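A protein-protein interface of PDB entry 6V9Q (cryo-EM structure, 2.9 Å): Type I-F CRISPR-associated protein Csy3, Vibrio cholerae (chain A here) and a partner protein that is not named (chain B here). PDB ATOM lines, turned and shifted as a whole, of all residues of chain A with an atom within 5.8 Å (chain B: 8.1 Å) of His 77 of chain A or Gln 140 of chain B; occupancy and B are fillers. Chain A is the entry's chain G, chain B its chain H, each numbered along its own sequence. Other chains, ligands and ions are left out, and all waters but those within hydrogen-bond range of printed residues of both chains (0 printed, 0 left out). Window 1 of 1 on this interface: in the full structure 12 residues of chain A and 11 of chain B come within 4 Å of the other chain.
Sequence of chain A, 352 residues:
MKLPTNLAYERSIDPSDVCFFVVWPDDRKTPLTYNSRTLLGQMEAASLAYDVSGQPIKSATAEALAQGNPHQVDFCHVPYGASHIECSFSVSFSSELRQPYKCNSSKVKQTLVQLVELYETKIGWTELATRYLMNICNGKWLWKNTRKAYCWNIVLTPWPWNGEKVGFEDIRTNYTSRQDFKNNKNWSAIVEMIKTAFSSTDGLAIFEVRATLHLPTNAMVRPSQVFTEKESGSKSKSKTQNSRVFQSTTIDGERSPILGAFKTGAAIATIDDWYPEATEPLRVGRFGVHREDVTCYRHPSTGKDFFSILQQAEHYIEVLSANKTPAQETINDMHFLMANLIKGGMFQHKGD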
ATOM      1  N   LEU A  32      16.102  17.819  -4.599  1.00  0.00           N
ATOM      2  CA  LEU A  32      14.806  18.341  -4.193  1.00  0.00           C
ATOM      3  C   LEU A  32      14.976  19.484  -3.203  1.00  0.00           C
ATOM      4  O   LEU A  32      15.900  19.481  -2.393  1.00  0.00           O
ATOM      5  CB  LEU A  32      13.984  17.210  -3.580  1.00  0.00           C
ATOM      6  CG  LEU A  32      12.566  17.429  -3.077  1.00  0.00           C
ATOM      7  CD1 LEU A  32      11.655  17.864  -4.189  1.00  0.00           C
ATOM      8  CD2 LEU A  32      12.058  16.153  -2.462  1.00  0.00           C
ATOM      9  N   THR A  33      14.105  20.485  -3.291  1.00  0.00           N
ATOM     10  CA  THR A  33      14.153  21.658  -2.427  1.00  0.00           C
ATOM     11  C   THR A  33      12.805  21.842  -1.746  1.00  0.00           C
ATOM     12  O   THR A  33      11.831  21.161  -2.064  1.00  0.00           O
ATOM     13  CB  THR A  33      14.519  22.923  -3.211  1.00  0.00           C
ATOM     14  OG1 THR A  33      13.558  23.125  -4.250  1.00  0.00           O
ATOM     15  CG2 THR A  33      15.896  22.804  -3.826  1.00  0.00           C
ATOM     16  N   TYR A  34      12.744  22.780  -0.803  1.00  0.00           N
ATOM     17  CA  TYR A  34      11.517  23.002  -0.047  1.00  0.00           C
ATOM     18  C   TYR A  34      11.399  24.482   0.305  1.00  0.00           C
ATOM     19  O   TYR A  34      12.306  25.274   0.046  1.00  0.00           O
ATOM     20  CB  TYR A  34      11.476  22.093   1.187  1.00  0.00           C
ATOM     21  CG  TYR A  34      12.531  22.342   2.231  1.00  0.00           C
ATOM     22  CD1 TYR A  34      13.778  21.745   2.145  1.00  0.00           C
ATOM     23  CD2 TYR A  34      12.263  23.131   3.330  1.00  0.00           C
ATOM     24  CE1 TYR A  34      14.737  21.947   3.112  1.00  0.00           C
ATOM     25  CE2 TYR A  34      13.216  23.349   4.296  1.00  0.00           C
ATOM     26  CZ  TYR A  34      14.446  22.746   4.186  1.00  0.00           C
ATOM     27  OH  TYR A  34      15.399  22.960   5.148  1.00  0.00           O
ATOM     28  N   ASN A  35      10.272  24.846   0.919  1.00  0.00           N
ATOM     29  CA  ASN A  35       9.919  26.221   1.244  1.00  0.00           C
ATOM     30  C   ASN A  35       9.948  26.435   2.749  1.00  0.00           C
ATOM     31  O   ASN A  35      10.065  25.493   3.531  1.00  0.00           O
ATOM     32  CB  ASN A  35       8.521  26.576   0.729  1.00  0.00           C
ATOM     33  CG  ASN A  35       8.481  26.771  -0.762  1.00  0.00           C
ATOM     34  OD1 ASN A  35       9.347  27.427  -1.333  1.00  0.00           O
ATOM     35  ND2 ASN A  35       7.470  26.201  -1.407  1.00  0.00           N
ATOM     36  N   PHE A  75       7.437  23.133   3.888  1.00  0.00           N
ATOM     37  CA  PHE A  75       6.626  22.273   3.044  1.00  0.00           C
ATOM     38  C   PHE A  75       7.469  21.825   1.868  1.00  0.00           C
ATOM     39  O   PHE A  75       8.147  22.642   1.240  1.00  0.00           O
ATOM     40  CB  PHE A  75       5.361  22.980   2.546  1.00  0.00           C
ATOM     41  CG  PHE A  75       4.396  22.056   1.857  1.00  0.00           C
ATOM     42  CD1 PHE A  75       3.530  21.268   2.602  1.00  0.00           C
ATOM     43  CD2 PHE A  75       4.385  21.933   0.470  1.00  0.00           C
ATOM     44  CE1 PHE A  75       2.651  20.402   1.976  1.00  0.00           C
ATOM     45  CE2 PHE A  75       3.515  21.055  -0.160  1.00  0.00           C
ATOM     46  CZ  PHE A  75       2.647  20.302   0.587  1.00  0.00           C
ATOM     47  N   CYS A  76       7.421  20.537   1.565  1.00  0.00           N
ATOM     48  CA  CYS A  76       8.180  19.987   0.460  1.00  0.00           C
ATOM     49  C   CYS A  76       7.237  19.206  -0.437  1.00  0.00           C
ATOM     50  O   CYS A  76       6.440  18.399   0.041  1.00  0.00           O
ATOM     51  CB  CYS A  76       9.310  19.096   0.963  1.00  0.00           C
ATOM     52  SG  CYS A  76      10.535  18.697  -0.275  1.00  0.00           S
ATOM     53  N   HIS A  77       7.325  19.457  -1.737  1.00  0.00           N
ATOM     54  CA  HIS A  77       6.436  18.822  -2.693  1.00  0.00           C
ATOM     55  C   HIS A  77       7.217  18.536  -3.959  1.00  0.00           C
ATOM     56  O   HIS A  77       8.261  19.137  -4.217  1.00  0.00           O
ATOM     57  CB  HIS A  77       5.225  19.706  -3.000  1.00  0.00           C
ATOM     58  CG  HIS A  77       5.576  20.982  -3.707  1.00  0.00           C
ATOM     59  ND1 HIS A  77       6.140  22.061  -3.060  1.00  0.00           N
ATOM     60  CD2 HIS A  77       5.442  21.351  -5.003  1.00  0.00           C
ATOM     61  CE1 HIS A  77       6.343  23.036  -3.928  1.00  0.00           C
ATOM     62  NE2 HIS A  77       5.925  22.632  -5.115  1.00  0.00           N
ATOM     63  N   VAL A  78       6.702  17.606  -4.744  1.00  0.00           N
ATOM     64  CA  VAL A  78       7.327  17.259  -6.018  1.00  0.00           C
ATOM     65  C   VAL A  78       7.069  18.395  -7.003  1.00  0.00           C
ATOM     66  O   VAL A  78       5.939  18.900  -7.059  1.00  0.00           O
ATOM     67  CB  VAL A  78       6.763  15.946  -6.541  1.00  0.00           C
ATOM     68  CG1 VAL A  78       7.519  15.478  -7.764  1.00  0.00           C
ATOM     69  CG2 VAL A  78       6.759  14.900  -5.458  1.00  0.00           C
ATOM     70  N   PRO A  79       8.069  18.844  -7.757  1.00  0.00           N
ATOM     71  CA  PRO A  79       7.827  19.871  -8.776  1.00  0.00           C
ATOM     72  C   PRO A  79       6.934  19.349  -9.893  1.00  0.00           C
ATOM     73  O   PRO A  79       6.697  18.147 -10.027  1.00  0.00           O
ATOM     74  CB  PRO A  79       9.232  20.196  -9.278  1.00  0.00           C
ATOM     75  CG  PRO A  79      10.125  19.812  -8.168  1.00  0.00           C
ATOM     76  CD  PRO A  79       9.506  18.606  -7.559  1.00  0.00           C
ATOM     77  N   ASN A 218       2.307  16.689  -8.122  1.00  0.00           N
ATOM     78  CA  ASN A 218       2.417  17.585  -6.964  1.00  0.00           C
ATOM     79  C   ASN A 218       2.071  16.845  -5.670  1.00  0.00           C
ATOM     80  O   ASN A 218       1.129  17.191  -4.956  1.00  0.00           O
ATOM     81  CB  ASN A 218       1.553  18.840  -7.145  1.00  0.00           C
ATOM     82  CG  ASN A 218       1.868  19.930  -6.135  1.00  0.00           C
ATOM     83  OD1 ASN A 218       2.782  19.804  -5.329  1.00  0.00           O
ATOM     84  ND2 ASN A 218       1.077  20.987  -6.150  1.00  0.00           N
ATOM     85  N   ALA A 219       2.842  15.807  -5.379  1.00  0.00           N
ATOM     86  CA  ALA A 219       2.560  14.955  -4.240  1.00  0.00           C
ATOM     87  C   ALA A 219       3.399  15.349  -3.035  1.00  0.00           C
ATOM     88  O   ALA A 219       4.405  16.049  -3.140  1.00  0.00           O
ATOM     89  CB  ALA A 219       2.812  13.491  -4.586  1.00  0.00           C
ATOM     90  N   MET A 220       2.951  14.890  -1.876  1.00  0.00           N
ATOM     91  CA  MET A 220       3.664  15.087  -0.627  1.00  0.00           C
ATOM     92  C   MET A 220       4.959  14.291  -0.616  1.00  0.00           C
ATOM     93  O   MET A 220       5.037  13.187  -1.157  1.00  0.00           O
ATOM     94  CB  MET A 220       2.800  14.611   0.534  1.00  0.00           C
ATOM     95  CG  MET A 220       1.503  15.339   0.712  1.00  0.00           C
ATOM     96  SD  MET A 220       1.812  16.984   1.303  1.00  0.00           S
ATOM     97  CE  MET A 220       2.435  16.554   2.906  1.00  0.00           C
ATOM     98  N   VAL A 221       5.983  14.856   0.016  1.00  0.00           N
ATOM     99  CA  VAL A 221       7.120  14.094   0.516  1.00  0.00           C
ATOM    100  C   VAL A 221       7.333  14.488   1.969  1.00  0.00           C
ATOM    101  O   VAL A 221       7.241  15.666   2.328  1.00  0.00           O
ATOM    102  CB  VAL A 221       8.401  14.295  -0.324  1.00  0.00           C
ATOM    103  CG1 VAL A 221       8.281  13.597  -1.663  1.00  0.00           C
ATOM    104  CG2 VAL A 221       8.617  15.720  -0.591  1.00  0.00           C
ATOM    105  N   LEU B 110       0.421  31.285  -2.635  1.00  0.00           N
ATOM    106  CA  LEU B 110       1.659  30.919  -1.958  1.00  0.00           C
ATOM    107  C   LEU B 110       1.675  29.481  -1.483  1.00  0.00           C
ATOM    108  O   LEU B 110       2.752  28.981  -1.149  1.00  0.00           O
ATOM    109  CB  LEU B 110       1.920  31.838  -0.769  1.00  0.00           C
ATOM    110  CG  LEU B 110       2.259  33.282  -1.102  1.00  0.00           C
ATOM    111  CD1 LEU B 110       2.464  34.057   0.180  1.00  0.00           C
ATOM    112  CD2 LEU B 110       3.489  33.339  -1.980  1.00  0.00           C
ATOM    113  N   THR B 111       0.530  28.814  -1.420  1.00  0.00           N
ATOM    114  CA  THR B 111       0.532  27.395  -1.123  1.00  0.00           C
ATOM    115  C   THR B 111       0.999  26.616  -2.344  1.00  0.00           C
ATOM    116  O   THR B 111       0.825  27.039  -3.488  1.00  0.00           O
ATOM    117  CB  THR B 111      -0.852  26.922  -0.697  1.00  0.00           C
ATOM    118  OG1 THR B 111      -1.777  27.119  -1.771  1.00  0.00           O
ATOM    119  CG2 THR B 111      -1.317  27.699   0.513  1.00  0.00           C
ATOM    120  N   ALA B 112       1.587  25.448  -2.081  1.00  0.00           N
ATOM    121  CA  ALA B 112       2.279  24.710  -3.132  1.00  0.00           C
ATOM    122  C   ALA B 112       1.305  24.023  -4.075  1.00  0.00           C
ATOM    123  O   ALA B 112       1.678  23.636  -5.188  1.00  0.00           O
ATOM    124  CB  ALA B 112       3.222  23.694  -2.509  1.00  0.00           C
ATOM    125  N   ALA B 113       0.060  23.839  -3.644  1.00  0.00           N
ATOM    126  CA  ALA B 113      -0.974  23.430  -4.582  1.00  0.00           C
ATOM    127  C   ALA B 113      -1.316  24.558  -5.539  1.00  0.00           C
ATOM    128  O   ALA B 113      -1.681  24.304  -6.691  1.00  0.00           O
ATOM    129  CB  ALA B 113      -2.219  22.976  -3.829  1.00  0.00           C
ATOM    130  N   GLY B 114      -1.191  25.804  -5.079  1.00  0.00           N
ATOM    131  CA  GLY B 114      -1.494  26.937  -5.935  1.00  0.00           C
ATOM    132  C   GLY B 114      -0.337  27.312  -6.834  1.00  0.00           C
ATOM    133  O   GLY B 114      -0.525  27.925  -7.887  1.00  0.00           O
ATOM    134  N   LEU B 115       0.880  26.962  -6.422  1.00  0.00           N
ATOM    135  CA  LEU B 115       2.038  27.148  -7.285  1.00  0.00           C
ATOM    136  C   LEU B 115       1.971  26.238  -8.501  1.00  0.00           C
ATOM    137  O   LEU B 115       2.477  26.593  -9.567  1.00  0.00           O
ATOM    138  CB  LEU B 115       3.320  26.884  -6.499  1.00  0.00           C
ATOM    139  CG  LEU B 115       3.624  27.830  -5.338  1.00  0.00           C
ATOM    140  CD1 LEU B 115       4.789  27.302  -4.527  1.00  0.00           C
ATOM    141  CD2 LEU B 115       3.933  29.217  -5.854  1.00  0.00           C
ATOM    142  N   ALA B 116       1.343  25.070  -8.366  1.00  0.00           N
ATOM    143  CA  ALA B 116       1.200  24.170  -9.504  1.00  0.00           C
ATOM    144  C   ALA B 116       0.044  24.592 -10.401  1.00  0.00           C
ATOM    145  O   ALA B 116       0.030  24.280 -11.595  1.00  0.00           O
ATOM    146  CB  ALA B 116       1.009  22.738  -9.020  1.00  0.00           C
ATOM    147  N   SER B 137      12.744  24.960 -15.306  1.00  0.00           N
ATOM    148  CA  SER B 137      13.408  26.251 -15.193  1.00  0.00           C
ATOM    149  C   SER B 137      12.891  27.029 -13.993  1.00  0.00           C
ATOM    150  O   SER B 137      13.585  27.903 -13.465  1.00  0.00           O
ATOM    151  CB  SER B 137      13.205  27.052 -16.475  1.00  0.00           C
ATOM    152  OG  SER B 137      11.837  27.378 -16.642  1.00  0.00           O
ATOM    153  N   PHE B 138      11.672  26.730 -13.556  1.00  0.00           N
ATOM    154  CA  PHE B 138      11.126  27.357 -12.369  1.00  0.00           C
ATOM    155  C   PHE B 138      11.801  26.802 -11.119  1.00  0.00           C
ATOM    156  O   PHE B 138      12.455  25.757 -11.138  1.00  0.00           O
ATOM    157  CB  PHE B 138       9.618  27.139 -12.295  1.00  0.00           C
ATOM    158  CG  PHE B 138       8.854  27.870 -13.349  1.00  0.00           C
ATOM    159  CD1 PHE B 138       8.518  29.201 -13.179  1.00  0.00           C
ATOM    160  CD2 PHE B 138       8.483  27.232 -14.519  1.00  0.00           C
ATOM    161  CE1 PHE B 138       7.814  29.884 -14.151  1.00  0.00           C
ATOM    162  CE2 PHE B 138       7.782  27.907 -15.495  1.00  0.00           C
ATOM    163  CZ  PHE B 138       7.445  29.234 -15.311  1.00  0.00           C
ATOM    164  N   ALA B 139      11.628  27.524 -10.019  1.00  0.00           N
ATOM    165  CA  ALA B 139      12.230  27.149  -8.753  1.00  0.00           C
ATOM    166  C   ALA B 139      11.409  27.771  -7.639  1.00  0.00           C
ATOM    167  O   ALA B 139      10.709  28.766  -7.839  1.00  0.00           O
ATOM    168  CB  ALA B 139      13.692  27.595  -8.665  1.00  0.00           C
ATOM    169  N   GLN B 140      11.500  27.169  -6.463  1.00  0.00           N
ATOM    170  CA  GLN B 140      10.716  27.642  -5.340  1.00  0.00           C
ATOM    171  C   GLN B 140      11.388  28.860  -4.722  1.00  0.00           C
ATOM    172  O   GLN B 140      12.565  29.133  -4.965  1.00  0.00           O
ATOM    173  CB  GLN B 140      10.566  26.529  -4.312  1.00  0.00           C
ATOM    174  CG  GLN B 140      10.000  25.262  -4.916  1.00  0.00           C
ATOM    175  CD  GLN B 140       9.850  24.161  -3.907  1.00  0.00           C
ATOM    176  OE1 GLN B 140      10.087  24.364  -2.721  1.00  0.00           O
ATOM    177  NE2 GLN B 140       9.501  22.966  -4.376  1.00  0.00           N
ATOM    178  N   LYS B 141      10.626  29.603  -3.923  1.00  0.00           N
ATOM    179  CA  LYS B 141      11.179  30.799  -3.299  1.00  0.00           C
ATOM    180  C   LYS B 141      12.135  30.433  -2.174  1.00  0.00           C
ATOM    181  O   LYS B 141      13.100  31.161  -1.906  1.00  0.00           O
ATOM    182  CB  LYS B 141      10.053  31.689  -2.773  1.00  0.00           C
ATOM    183  CG  LYS B 141       9.199  32.326  -3.847  1.00  0.00           C
ATOM    184  CD  LYS B 141       8.118  33.206  -3.238  1.00  0.00           C
ATOM    185  CE  LYS B 141       7.241  33.840  -4.311  1.00  0.00           C
ATOM    186  NZ  LYS B 141       6.166  34.691  -3.728  1.00  0.00           N
ATOM    187  N   GLU B 142      11.810  29.358  -1.441  1.00  0.00           N
ATOM    188  CA  GLU B 142      12.552  28.722  -0.348  1.00  0.00           C
ATOM    189  C   GLU B 142      12.575  29.547   0.934  1.00  0.00           C
ATOM    190  O   GLU B 142      12.951  29.030   1.988  1.00  0.00           O
ATOM    191  CB  GLU B 142      13.992  28.382  -0.746  1.00  0.00           C
ATOM    192  CG  GLU B 142      14.118  27.348  -1.835  1.00  0.00           C
ATOM    193  CD  GLU B 142      15.558  27.001  -2.125  1.00  0.00           C
ATOM    194  OE1 GLU B 142      16.454  27.641  -1.537  1.00  0.00           O
ATOM    195  OE2 GLU B 142      15.798  26.091  -2.942  1.00  0.00           O
ATOM    196  N   HIS B 143      12.130  30.804   0.866  1.00  0.00           N
ATOM    197  CA  HIS B 143      12.055  31.689   2.027  1.00  0.00           C
ATOM    198  C   HIS B 143      10.940  32.680   1.715  1.00  0.00           C
ATOM    199  O   HIS B 143      11.100  33.527   0.834  1.00  0.00           O
ATOM    200  CB  HIS B 143      13.367  32.410   2.294  1.00  0.00           C
ATOM    201  CG  HIS B 143      14.467  31.525   2.784  1.00  0.00           C
ATOM    202  ND1 HIS B 143      14.514  31.045   4.074  1.00  0.00           N
ATOM    203  CD2 HIS B 143      15.551  31.017   2.152  1.00  0.00           C
ATOM    204  CE1 HIS B 143      15.587  30.288   4.219  1.00  0.00           C
ATOM    205  NE2 HIS B 143      16.232  30.255   3.067  1.00  0.00           N
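The backbone carbonyl oxygen of Thr 33 of chain A sits at hydrogen-bond distance from the side-chain sulfur of Cys 76 of chain A, at 3.3 Å.
The backbone NH (N) of Asn 35 of chain A is in hydrogen-bond range of the backbone carbonyl oxygen (O) of Phe 75 of chain A (3.1 Å).
Of chain B, only Ala 112 (3.4 Å) and Gln 140 (3.2 Å) come within 4 Å of His 77 of chain A.
Of chain A, only Thr 33 (3.7 Å), Tyr 34 (3.3 Å), Asn 35 (3.3 Å) and His 77 (3.2 Å) come within 4 Å of Gln 140 of chain B.
No residue of chain B comes within 4 Å of Cys 76 of chain A.
Of the printed residues of chain A, Ala 112 of chain B touches Phe 75, His 77 and Asn 218.
Of the printed residues of chain A, Glu 142 of chain B touches Thr 33, Tyr 34 and Asn 35.
Leu 115 of chain B touches none of the printed residues of chain A.
Thr 111 of chain B touches none of the printed residues of chain A.
The nearest residue of chain B that does not touch His 77 of chain A is Leu 115 of chain B (4.6 Å).
The nearest residue of chain A that does not touch Gln 140 of chain B is Phe 75 of chain A (4.7 Å).
Of the 14 printed residues of chain B, 6 touch a printed residue of chain A.
Printed residues of chain B that touch a printed residue of chain A: Ala 112, Ala 113, Ala 116, Gln 140, Lys 141 and Glu 142.
Hydrophobic or aromatic side chains of chain A that line the printed part of chain B: Phe 75 and His 77.
Among the printed residues, no Asp or Glu carboxylate lies within 4 Å of a Lys or Arg side-chain nitrogen of the other chain.
OD1 of Asn 35 of chain A lies close to OE1 of Gln 140 of chain B, at 3.4 Å.
OD1 of Asn 35 of chain A is in hydrogen-bond range of N of Glu 142 of chain B (3.1 Å).
The side-chain amide nitrogen (ND2) of Asn 218 of chain A sits at hydrogen-bond distance from the backbone carbonyl oxygen (O) of Ala 112 of chain B.
Among the printed residues, pairs that only touch across the chains: His 77 of chain A with Gln 140 of chain B (3.2 Å), Tyr 34 of chain A with Gln 140 of chain B (3.3 Å), Tyr 34 of chain A with Glu 142 of chain B (3.3 Å), Asn 218 of chain A with Ala 116 of chain B (3.4 Å), His 77 of chain A with Ala 112 of chain B (3.4 Å), Thr 33 of chain A with Glu 142 of chain B (3.4 Å), Phe 75 of chain A with Ala 112 of chain B (3.5 Å), Asn 218 of chain A with Ala 113 of chain B (3.6 Å), Asn 35 of chain A with Lys 141 of chain B (3.6 Å) and Thr 33 of chain A with Gln 140 of chain B (3.7 Å).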
